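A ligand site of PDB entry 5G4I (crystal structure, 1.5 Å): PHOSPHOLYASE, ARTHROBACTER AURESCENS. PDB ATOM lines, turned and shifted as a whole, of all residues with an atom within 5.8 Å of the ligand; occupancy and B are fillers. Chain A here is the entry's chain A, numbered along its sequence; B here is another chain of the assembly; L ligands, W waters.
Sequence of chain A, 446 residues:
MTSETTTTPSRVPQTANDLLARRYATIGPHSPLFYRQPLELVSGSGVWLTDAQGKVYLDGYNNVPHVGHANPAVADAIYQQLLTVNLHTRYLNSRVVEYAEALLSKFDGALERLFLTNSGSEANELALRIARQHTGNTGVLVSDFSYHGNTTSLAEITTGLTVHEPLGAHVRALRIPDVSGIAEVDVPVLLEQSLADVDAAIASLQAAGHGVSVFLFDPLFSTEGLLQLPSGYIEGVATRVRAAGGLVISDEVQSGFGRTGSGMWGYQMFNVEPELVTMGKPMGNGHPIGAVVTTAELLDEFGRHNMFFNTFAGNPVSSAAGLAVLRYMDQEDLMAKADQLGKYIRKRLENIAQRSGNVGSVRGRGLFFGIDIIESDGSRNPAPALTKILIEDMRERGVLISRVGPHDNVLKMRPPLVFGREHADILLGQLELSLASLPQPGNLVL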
ATOM      1  N   SER A 119       8.836   8.378   9.262  1.00  0.00           N
ATOM      2  CA  SER A 119       8.907   8.723   7.808  1.00  0.00           C
ATOM      3  C   SER A 119      10.313   9.280   7.453  1.00  0.00           C
ATOM      4  O   SER A 119      11.040   9.791   8.341  1.00  0.00           O
ATOM      5  CB  SER A 119       7.847   9.720   7.375  1.00  0.00           C
ATOM      6  OG  SER A 119       8.096  11.031   7.907  1.00  0.00           O
ATOM      7  N   GLY A 120      10.655   9.253   6.186  1.00  0.00           N
ATOM      8  CA  GLY A 120      11.901   9.927   5.709  1.00  0.00           C
ATOM      9  C   GLY A 120      11.829  11.405   5.942  1.00  0.00           C
ATOM     10  O   GLY A 120      12.883  12.036   6.324  1.00  0.00           O
ATOM     11  N   SER A 121      10.674  12.066   5.695  1.00  0.00           N
ATOM     12  CA  SER A 121      10.578  13.569   5.976  1.00  0.00           C
ATOM     13  C   SER A 121      10.844  13.819   7.451  1.00  0.00           C
ATOM     14  O   SER A 121      11.510  14.828   7.802  1.00  0.00           O
ATOM     15  CB  SER A 121       9.201  14.190   5.485  1.00  0.00           C
ATOM     16  OG  SER A 121       9.114  14.159   4.076  1.00  0.00           O
ATOM     17  N   GLU A 122      10.250  13.042   8.349  1.00  0.00           N
ATOM     18  CA  GLU A 122      10.510  13.258   9.816  1.00  0.00           C
ATOM     19  C   GLU A 122      11.985  13.121  10.076  1.00  0.00           C
ATOM     20  O   GLU A 122      12.552  13.903  10.932  1.00  0.00           O
ATOM     21  CB  GLU A 122       9.674  12.349  10.718  1.00  0.00           C
ATOM     22  CG  GLU A 122       8.210  12.658  10.873  1.00  0.00           C
ATOM     23  CD  GLU A 122       7.581  11.980  12.107  1.00  0.00           C
ATOM     24  OE1 GLU A 122       7.870  10.756  12.407  1.00  0.00           O
ATOM     25  OE2 GLU A 122       6.767  12.672  12.843  1.00  0.00           O
ATOM     26  N   ASN A 124      14.705  13.637   7.976  1.00  0.00           N
ATOM     27  CA  ASN A 124      15.475  14.773   7.458  1.00  0.00           C
ATOM     28  C   ASN A 124      15.116  16.062   8.219  1.00  0.00           C
ATOM     29  O   ASN A 124      16.045  16.886   8.474  1.00  0.00           O
ATOM     30  CB  ASN A 124      15.278  14.973   5.935  1.00  0.00           C
ATOM     31  CG  ASN A 124      16.079  14.014   5.086  1.00  0.00           C
ATOM     32  OD1 ASN A 124      17.232  13.699   5.439  1.00  0.00           O
ATOM     33  ND2 ASN A 124      15.564  13.655   3.932  1.00  0.00           N
ATOM     34  N   TYR A 147      15.205  16.521  -3.881  1.00  0.00           N
ATOM     35  CA  TYR A 147      13.986  16.448  -3.078  1.00  0.00           C
ATOM     36  C   TYR A 147      14.245  15.598  -1.810  1.00  0.00           C
ATOM     37  O   TYR A 147      14.660  14.434  -1.901  1.00  0.00           O
ATOM     38  CB  TYR A 147      12.789  15.895  -3.861  1.00  0.00           C
ATOM     39  CG  TYR A 147      11.548  15.721  -2.993  1.00  0.00           C
ATOM     40  CD1 TYR A 147      10.827  16.799  -2.538  1.00  0.00           C
ATOM     41  CD2 TYR A 147      11.156  14.445  -2.528  1.00  0.00           C
ATOM     42  CE1 TYR A 147       9.744  16.691  -1.715  1.00  0.00           C
ATOM     43  CE2 TYR A 147      10.017  14.295  -1.729  1.00  0.00           C
ATOM     44  CZ  TYR A 147       9.325  15.413  -1.310  1.00  0.00           C
ATOM     45  OH  TYR A 147       8.244  15.297  -0.464  1.00  0.00           O
ATOM     46  N   HIS A 148      14.073  16.227  -0.641  1.00  0.00           N
ATOM     47  CA  HIS A 148      14.384  15.557   0.646  1.00  0.00           C
ATOM     48  C   HIS A 148      13.205  15.453   1.613  1.00  0.00           C
ATOM     49  O   HIS A 148      13.309  14.955   2.738  1.00  0.00           O
ATOM     50  CB  HIS A 148      15.607  16.306   1.312  1.00  0.00           C
ATOM     51  CG  HIS A 148      16.850  16.226   0.487  1.00  0.00           C
ATOM     52  ND1 HIS A 148      17.587  15.084   0.349  1.00  0.00           N
ATOM     53  CD2 HIS A 148      17.477  17.160  -0.280  1.00  0.00           C
ATOM     54  CE1 HIS A 148      18.592  15.312  -0.463  1.00  0.00           C
ATOM     55  NE2 HIS A 148      18.535  16.551  -0.902  1.00  0.00           N
ATOM     56  N   GLY A 149      12.014  15.890   1.201  1.00  0.00           N
ATOM     57  CA  GLY A 149      10.787  15.749   1.979  1.00  0.00           C
ATOM     58  C   GLY A 149       9.871  16.970   1.992  1.00  0.00           C
ATOM     59  O   GLY A 149      10.083  17.942   1.244  1.00  0.00           O
ATOM     60  N   ASN A 150       8.808  16.871   2.838  1.00  0.00           N
ATOM     61  CA  ASN A 150       7.600  17.685   2.643  1.00  0.00           C
ATOM     62  C   ASN A 150       7.190  18.621   3.803  1.00  0.00           C
ATOM     63  O   ASN A 150       6.037  19.145   3.820  1.00  0.00           O
ATOM     64  CB  ASN A 150       6.479  16.720   2.269  1.00  0.00           C
ATOM     65  CG  ASN A 150       6.204  15.751   3.381  1.00  0.00           C
ATOM     66  OD1 ASN A 150       6.401  16.038   4.566  1.00  0.00           O
ATOM     67  ND2 ASN A 150       5.760  14.515   3.032  1.00  0.00           N
ATOM     68  N   ASP A 218      21.617  12.943  -1.611  1.00  0.00           N
ATOM     69  CA  ASP A 218      21.371  11.533  -1.974  1.00  0.00           C
ATOM     70  C   ASP A 218      22.574  10.975  -2.673  1.00  0.00           C
ATOM     71  O   ASP A 218      22.916  11.468  -3.786  1.00  0.00           O
ATOM     72  CB  ASP A 218      20.133  11.461  -2.891  1.00  0.00           C
ATOM     73  CG  ASP A 218      19.957  10.165  -3.689  1.00  0.00           C
ATOM     74  OD1 ASP A 218      20.561   9.125  -3.303  1.00  0.00           O
ATOM     75  OD2 ASP A 218      19.186  10.229  -4.709  1.00  0.00           O
ATOM     76  N   ASP A 251      21.455  11.347   2.902  1.00  0.00           N
ATOM     77  CA  ASP A 251      20.034  10.925   2.827  1.00  0.00           C
ATOM     78  C   ASP A 251      20.049   9.573   2.073  1.00  0.00           C
ATOM     79  O   ASP A 251      20.335   9.540   0.889  1.00  0.00           O
ATOM     80  CB  ASP A 251      19.240  11.985   2.097  1.00  0.00           C
ATOM     81  CG  ASP A 251      17.771  11.625   1.893  1.00  0.00           C
ATOM     82  OD1 ASP A 251      17.445  10.441   1.963  1.00  0.00           O
ATOM     83  OD2 ASP A 251      16.972  12.553   1.561  1.00  0.00           O
ATOM     84  N   VAL A 253      17.494   7.445   1.861  1.00  0.00           N
ATOM     85  CA  VAL A 253      16.126   6.936   1.540  1.00  0.00           C
ATOM     86  C   VAL A 253      16.112   6.200   0.237  1.00  0.00           C
ATOM     87  O   VAL A 253      15.409   5.116   0.174  1.00  0.00           O
ATOM     88  CB  VAL A 253      15.066   8.094   1.594  1.00  0.00           C
ATOM     89  CG1 VAL A 253      13.716   7.584   1.113  1.00  0.00           C
ATOM     90  CG2 VAL A 253      14.977   8.678   2.970  1.00  0.00           C
ATOM     91  N   GLN A 254      16.823   6.631  -0.775  1.00  0.00           N
ATOM     92  CA  GLN A 254      16.919   5.945  -2.093  1.00  0.00           C
ATOM     93  C   GLN A 254      18.082   4.940  -2.198  1.00  0.00           C
ATOM     94  O   GLN A 254      17.938   3.925  -2.950  1.00  0.00           O
ATOM     95  CB  GLN A 254      17.113   6.934  -3.290  1.00  0.00           C
ATOM     96  CG  GLN A 254      15.997   7.922  -3.470  1.00  0.00           C
ATOM     97  CD  GLN A 254      14.743   7.292  -4.079  1.00  0.00           C
ATOM     98  OE1 GLN A 254      14.773   6.292  -4.740  1.00  0.00           O
ATOM     99  NE2 GLN A 254      13.650   7.923  -3.857  1.00  0.00           N
ATOM    100  N   GLY A 280      14.416   5.828   5.420  1.00  0.00           N
ATOM    101  CA  GLY A 280      12.945   5.678   5.393  1.00  0.00           C
ATOM    102  C   GLY A 280      12.640   4.590   4.355  1.00  0.00           C
ATOM    103  O   GLY A 280      13.224   3.504   4.361  1.00  0.00           O
ATOM    104  N   LYS A 281      11.754   4.924   3.394  1.00  0.00           N
ATOM    105  CA  LYS A 281      11.146   4.034   2.365  1.00  0.00           C
ATOM    106  C   LYS A 281      11.243   2.515   2.671  1.00  0.00           C
ATOM    107  O   LYS A 281      10.267   1.933   3.209  1.00  0.00           O
ATOM    108  CB  LYS A 281      11.490   4.525   0.970  1.00  0.00           C
ATOM    109  CG  LYS A 281      10.685   5.776   0.534  1.00  0.00           C
ATOM    110  CD  LYS A 281      10.950   6.192  -0.947  1.00  0.00           C
ATOM    111  CE  LYS A 281      10.115   7.450  -1.465  1.00  0.00           C
ATOM    112  NZ  LYS A 281      10.990   8.626  -1.233  1.00  0.00           N
ATOM    113  N   GLU B 122       3.453  15.429  12.155  1.00  0.00           N
ATOM    114  CA  GLU B 122       3.359  15.650  10.734  1.00  0.00           C
ATOM    115  C   GLU B 122       2.028  16.423  10.379  1.00  0.00           C
ATOM    116  O   GLU B 122       2.050  17.275   9.448  1.00  0.00           O
ATOM    117  CB  GLU B 122       3.393  14.355   9.885  1.00  0.00           C
ATOM    118  CG  GLU B 122       4.814  13.752   9.710  1.00  0.00           C
ATOM    119  CD  GLU B 122       4.880  12.723   8.599  1.00  0.00           C
ATOM    120  OE1 GLU B 122       3.906  11.893   8.365  1.00  0.00           O
ATOM    121  OE2 GLU B 122       5.943  12.698   7.860  1.00  0.00           O
ATOM    122  N   PHE B 309       3.335  15.327  -1.457  1.00  0.00           N
ATOM    123  CA  PHE B 309       3.220  13.869  -1.376  1.00  0.00           C
ATOM    124  C   PHE B 309       3.966  13.368  -0.137  1.00  0.00           C
ATOM    125  O   PHE B 309       5.090  13.840   0.168  1.00  0.00           O
ATOM    126  CB  PHE B 309       3.871  13.241  -2.639  1.00  0.00           C
ATOM    127  CG  PHE B 309       3.808  11.754  -2.693  1.00  0.00           C
ATOM    128  CD1 PHE B 309       2.586  11.113  -2.880  1.00  0.00           C
ATOM    129  CD2 PHE B 309       4.981  11.006  -2.631  1.00  0.00           C
ATOM    130  CE1 PHE B 309       2.558   9.683  -2.885  1.00  0.00           C
ATOM    131  CE2 PHE B 309       4.959   9.617  -2.718  1.00  0.00           C
ATOM    132  CZ  PHE B 309       3.762   8.956  -2.849  1.00  0.00           C
ATOM    133  N   ASN B 310       3.355  12.394   0.543  1.00  0.00           N
ATOM    134  CA  ASN B 310       3.857  11.729   1.791  1.00  0.00           C
ATOM    135  C   ASN B 310       3.859  10.252   1.444  1.00  0.00           C
ATOM    136  O   ASN B 310       2.738   9.648   1.269  1.00  0.00           O
ATOM    137  CB  ASN B 310       2.928  12.173   2.943  1.00  0.00           C
ATOM    138  CG  ASN B 310       3.222  11.468   4.283  1.00  0.00           C
ATOM    139  OD1 ASN B 310       3.589  10.270   4.299  1.00  0.00           O
ATOM    140  ND2 ASN B 310       3.106  12.198   5.348  1.00  0.00           N
ATOM    141  N   THR B 311       5.020   9.599   1.355  1.00  0.00           N
ATOM    142  CA  THR B 311       5.097   8.235   0.756  1.00  0.00           C
ATOM    143  C   THR B 311       4.290   7.181   1.516  1.00  0.00           C
ATOM    144  O   THR B 311       3.598   6.322   0.912  1.00  0.00           O
ATOM    145  CB  THR B 311       6.577   7.774   0.655  1.00  0.00           C
ATOM    146  OG1 THR B 311       7.343   8.760  -0.091  1.00  0.00           O
ATOM    147  CG2 THR B 311       6.648   6.423  -0.070  1.00  0.00           C
ATOM    148  N   PHE B 312       4.399   7.184   2.818  1.00  0.00           N
ATOM    149  CA  PHE B 312       3.682   6.178   3.642  1.00  0.00           C
ATOM    150  C   PHE B 312       2.215   6.554   3.908  1.00  0.00           C
ATOM    151  O   PHE B 312       1.371   5.628   4.237  1.00  0.00           O
ATOM    152  CB  PHE B 312       4.360   5.944   4.987  1.00  0.00           C
ATOM    153  CG  PHE B 312       5.772   5.384   4.882  1.00  0.00           C
ATOM    154  CD1 PHE B 312       6.109   4.287   4.069  1.00  0.00           C
ATOM    155  CD2 PHE B 312       6.782   5.900   5.678  1.00  0.00           C
ATOM    156  CE1 PHE B 312       7.410   3.741   4.022  1.00  0.00           C
ATOM    157  CE2 PHE B 312       8.070   5.349   5.635  1.00  0.00           C
ATOM    158  CZ  PHE B 312       8.366   4.248   4.812  1.00  0.00           C
HETATM  159  N1  LIG L   1      14.453  11.881   0.683  1.00  0.00           N
HETATM  160  C1  LIG L   1      14.535  11.063  -0.390  1.00  0.00           C
HETATM  161  C2  LIG L   1      15.847  10.907  -1.111  1.00  0.00           C
HETATM  162  C3  LIG L   1      13.339  10.333  -0.859  1.00  0.00           C
HETATM  163  O1  LIG L   1      13.397   9.505  -1.946  1.00  0.00           O
HETATM  164  C4  LIG L   1      12.074  10.528  -0.119  1.00  0.00           C
HETATM  165  C5  LIG L   1      10.828   9.837  -0.506  1.00  0.00           C
HETATM  166  C6  LIG L   1      12.118  11.451   1.044  1.00  0.00           C
HETATM  167  C7  LIG L   1      13.325  12.072   1.378  1.00  0.00           C
HETATM  168  C8  LIG L   1      10.874  11.711   1.872  1.00  0.00           C
HETATM  169  O2  LIG L   1      10.310  10.465   2.275  1.00  0.00           O
HETATM  170  P1  LIG L   1       8.831  10.406   2.926  1.00  0.00           P
HETATM  171  O3  LIG L   1       7.915  10.526   1.737  1.00  0.00           O
HETATM  172  O4  LIG L   1       8.786   9.065   3.615  1.00  0.00           O
HETATM  173  O5  LIG L   1       8.804  11.601   3.854  1.00  0.00           O
HETATM  174  O   HOH W   1       6.099   8.887   4.399  1.00  0.00           O
HETATM  175  O   HOH W   2       7.603  12.688  -0.070  1.00  0.00           O
HETATM  176  O   HOH W   3       6.109  12.164   4.820  1.00  0.00           O
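The side-chain hydroxyl (OG) of Ser 121 is in hydrogen-bond range of an oxygen (O5) of the ligand. The backbone NH (N) of Gly 120 sits at hydrogen-bond distance from an oxygen (O4) of the ligand. OG1 of Thr 311 of chain B is in hydrogen-bond range of O3 of the ligand (2.6 Å). OD2 of Asp 251 is in hydrogen-bond range of N1 of the ligand, at 2.8 Å. NZ of Lys 281 is bonded to C5 of the ligand, 1.4 Å away. An oxygen (O3) of the ligand sits at hydrogen-bond distance from the backbone NH (N) of Thr 311 of chain B. The side-chain amide nitrogen (NE2) of Gln 254 sits at hydrogen-bond distance from an oxygen (O1) of the ligand. N of Ser 121 lies within hydrogen-bond range of O5 of the ligand (2.7 Å).
The side-chain hydroxyl (OG) of Ser 121 sits at hydrogen-bond distance from the backbone NH (N) of Asn 150 (3.0 Å). OG of Ser 119 sits at hydrogen-bond distance from OE2 of Glu 122 of chain B (2.7 Å). A ring nitrogen (ND1) of His 148 sits at hydrogen-bond distance from the side-chain carboxylate of Asp 251. The backbone NH of Glu 122 of chain A sits at hydrogen-bond distance from the side-chain hydroxyl of Ser 119, at 3.0 Å. The side-chain carboxylate (OD2) of Asp 251 lies within hydrogen-bond range of the side-chain amide nitrogen (ND2) of Asn 124 (3.0 Å). The backbone carbonyl oxygen (O) of His 148 lies within hydrogen-bond range of the side-chain amide nitrogen (ND2) of Asn 124 (2.9 Å). The side-chain carboxylate (OD1) of Asp 251 lies within hydrogen-bond range of the backbone NH (N) of Val 253.
Ser 119 touches the ligand. Asn 124 touches the ligand (ND2 to C7, 3.7 Å). Tyr 147 touches the ligand. O of His 148 touches C7 of the ligand, 3.2 Å away. Val 253 touches the ligand (CG1 to C3, 3.4 Å). 11 residues have an atom within 4 Å of the ligand: Ser 119, Gly 120, Ser 121, Asn 124, Tyr 147, His 148, Asp 251, Val 253, Gln 254, Lys 281 and Thr 311 of chain B.
Water W1 lies within hydrogen-bond range of O4 of the ligand (2.8 Å), OD1 of Asn 310 of chain B (2.9 Å), N of Phe 312 of chain B (2.9 Å) and N of Thr 311 of chain B (3.3 Å). Water W2 lies within hydrogen-bond range of OH of Tyr 147 (2.7 Å), O of Phe 309 of chain B (2.8 Å) and O3 of the ligand (2.8 Å). Water W3 lies within hydrogen-bond range of an oxygen (O5) of the ligand (2.9 Å), the side-chain amide nitrogen (ND2) of Asn 150 (3.0 Å), the side-chain amide nitrogen (ND2) of Asn 310 of chain B (3.0 Å) and the side-chain carboxylate (OE2) of Glu 122 of chain B (3.1 Å).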
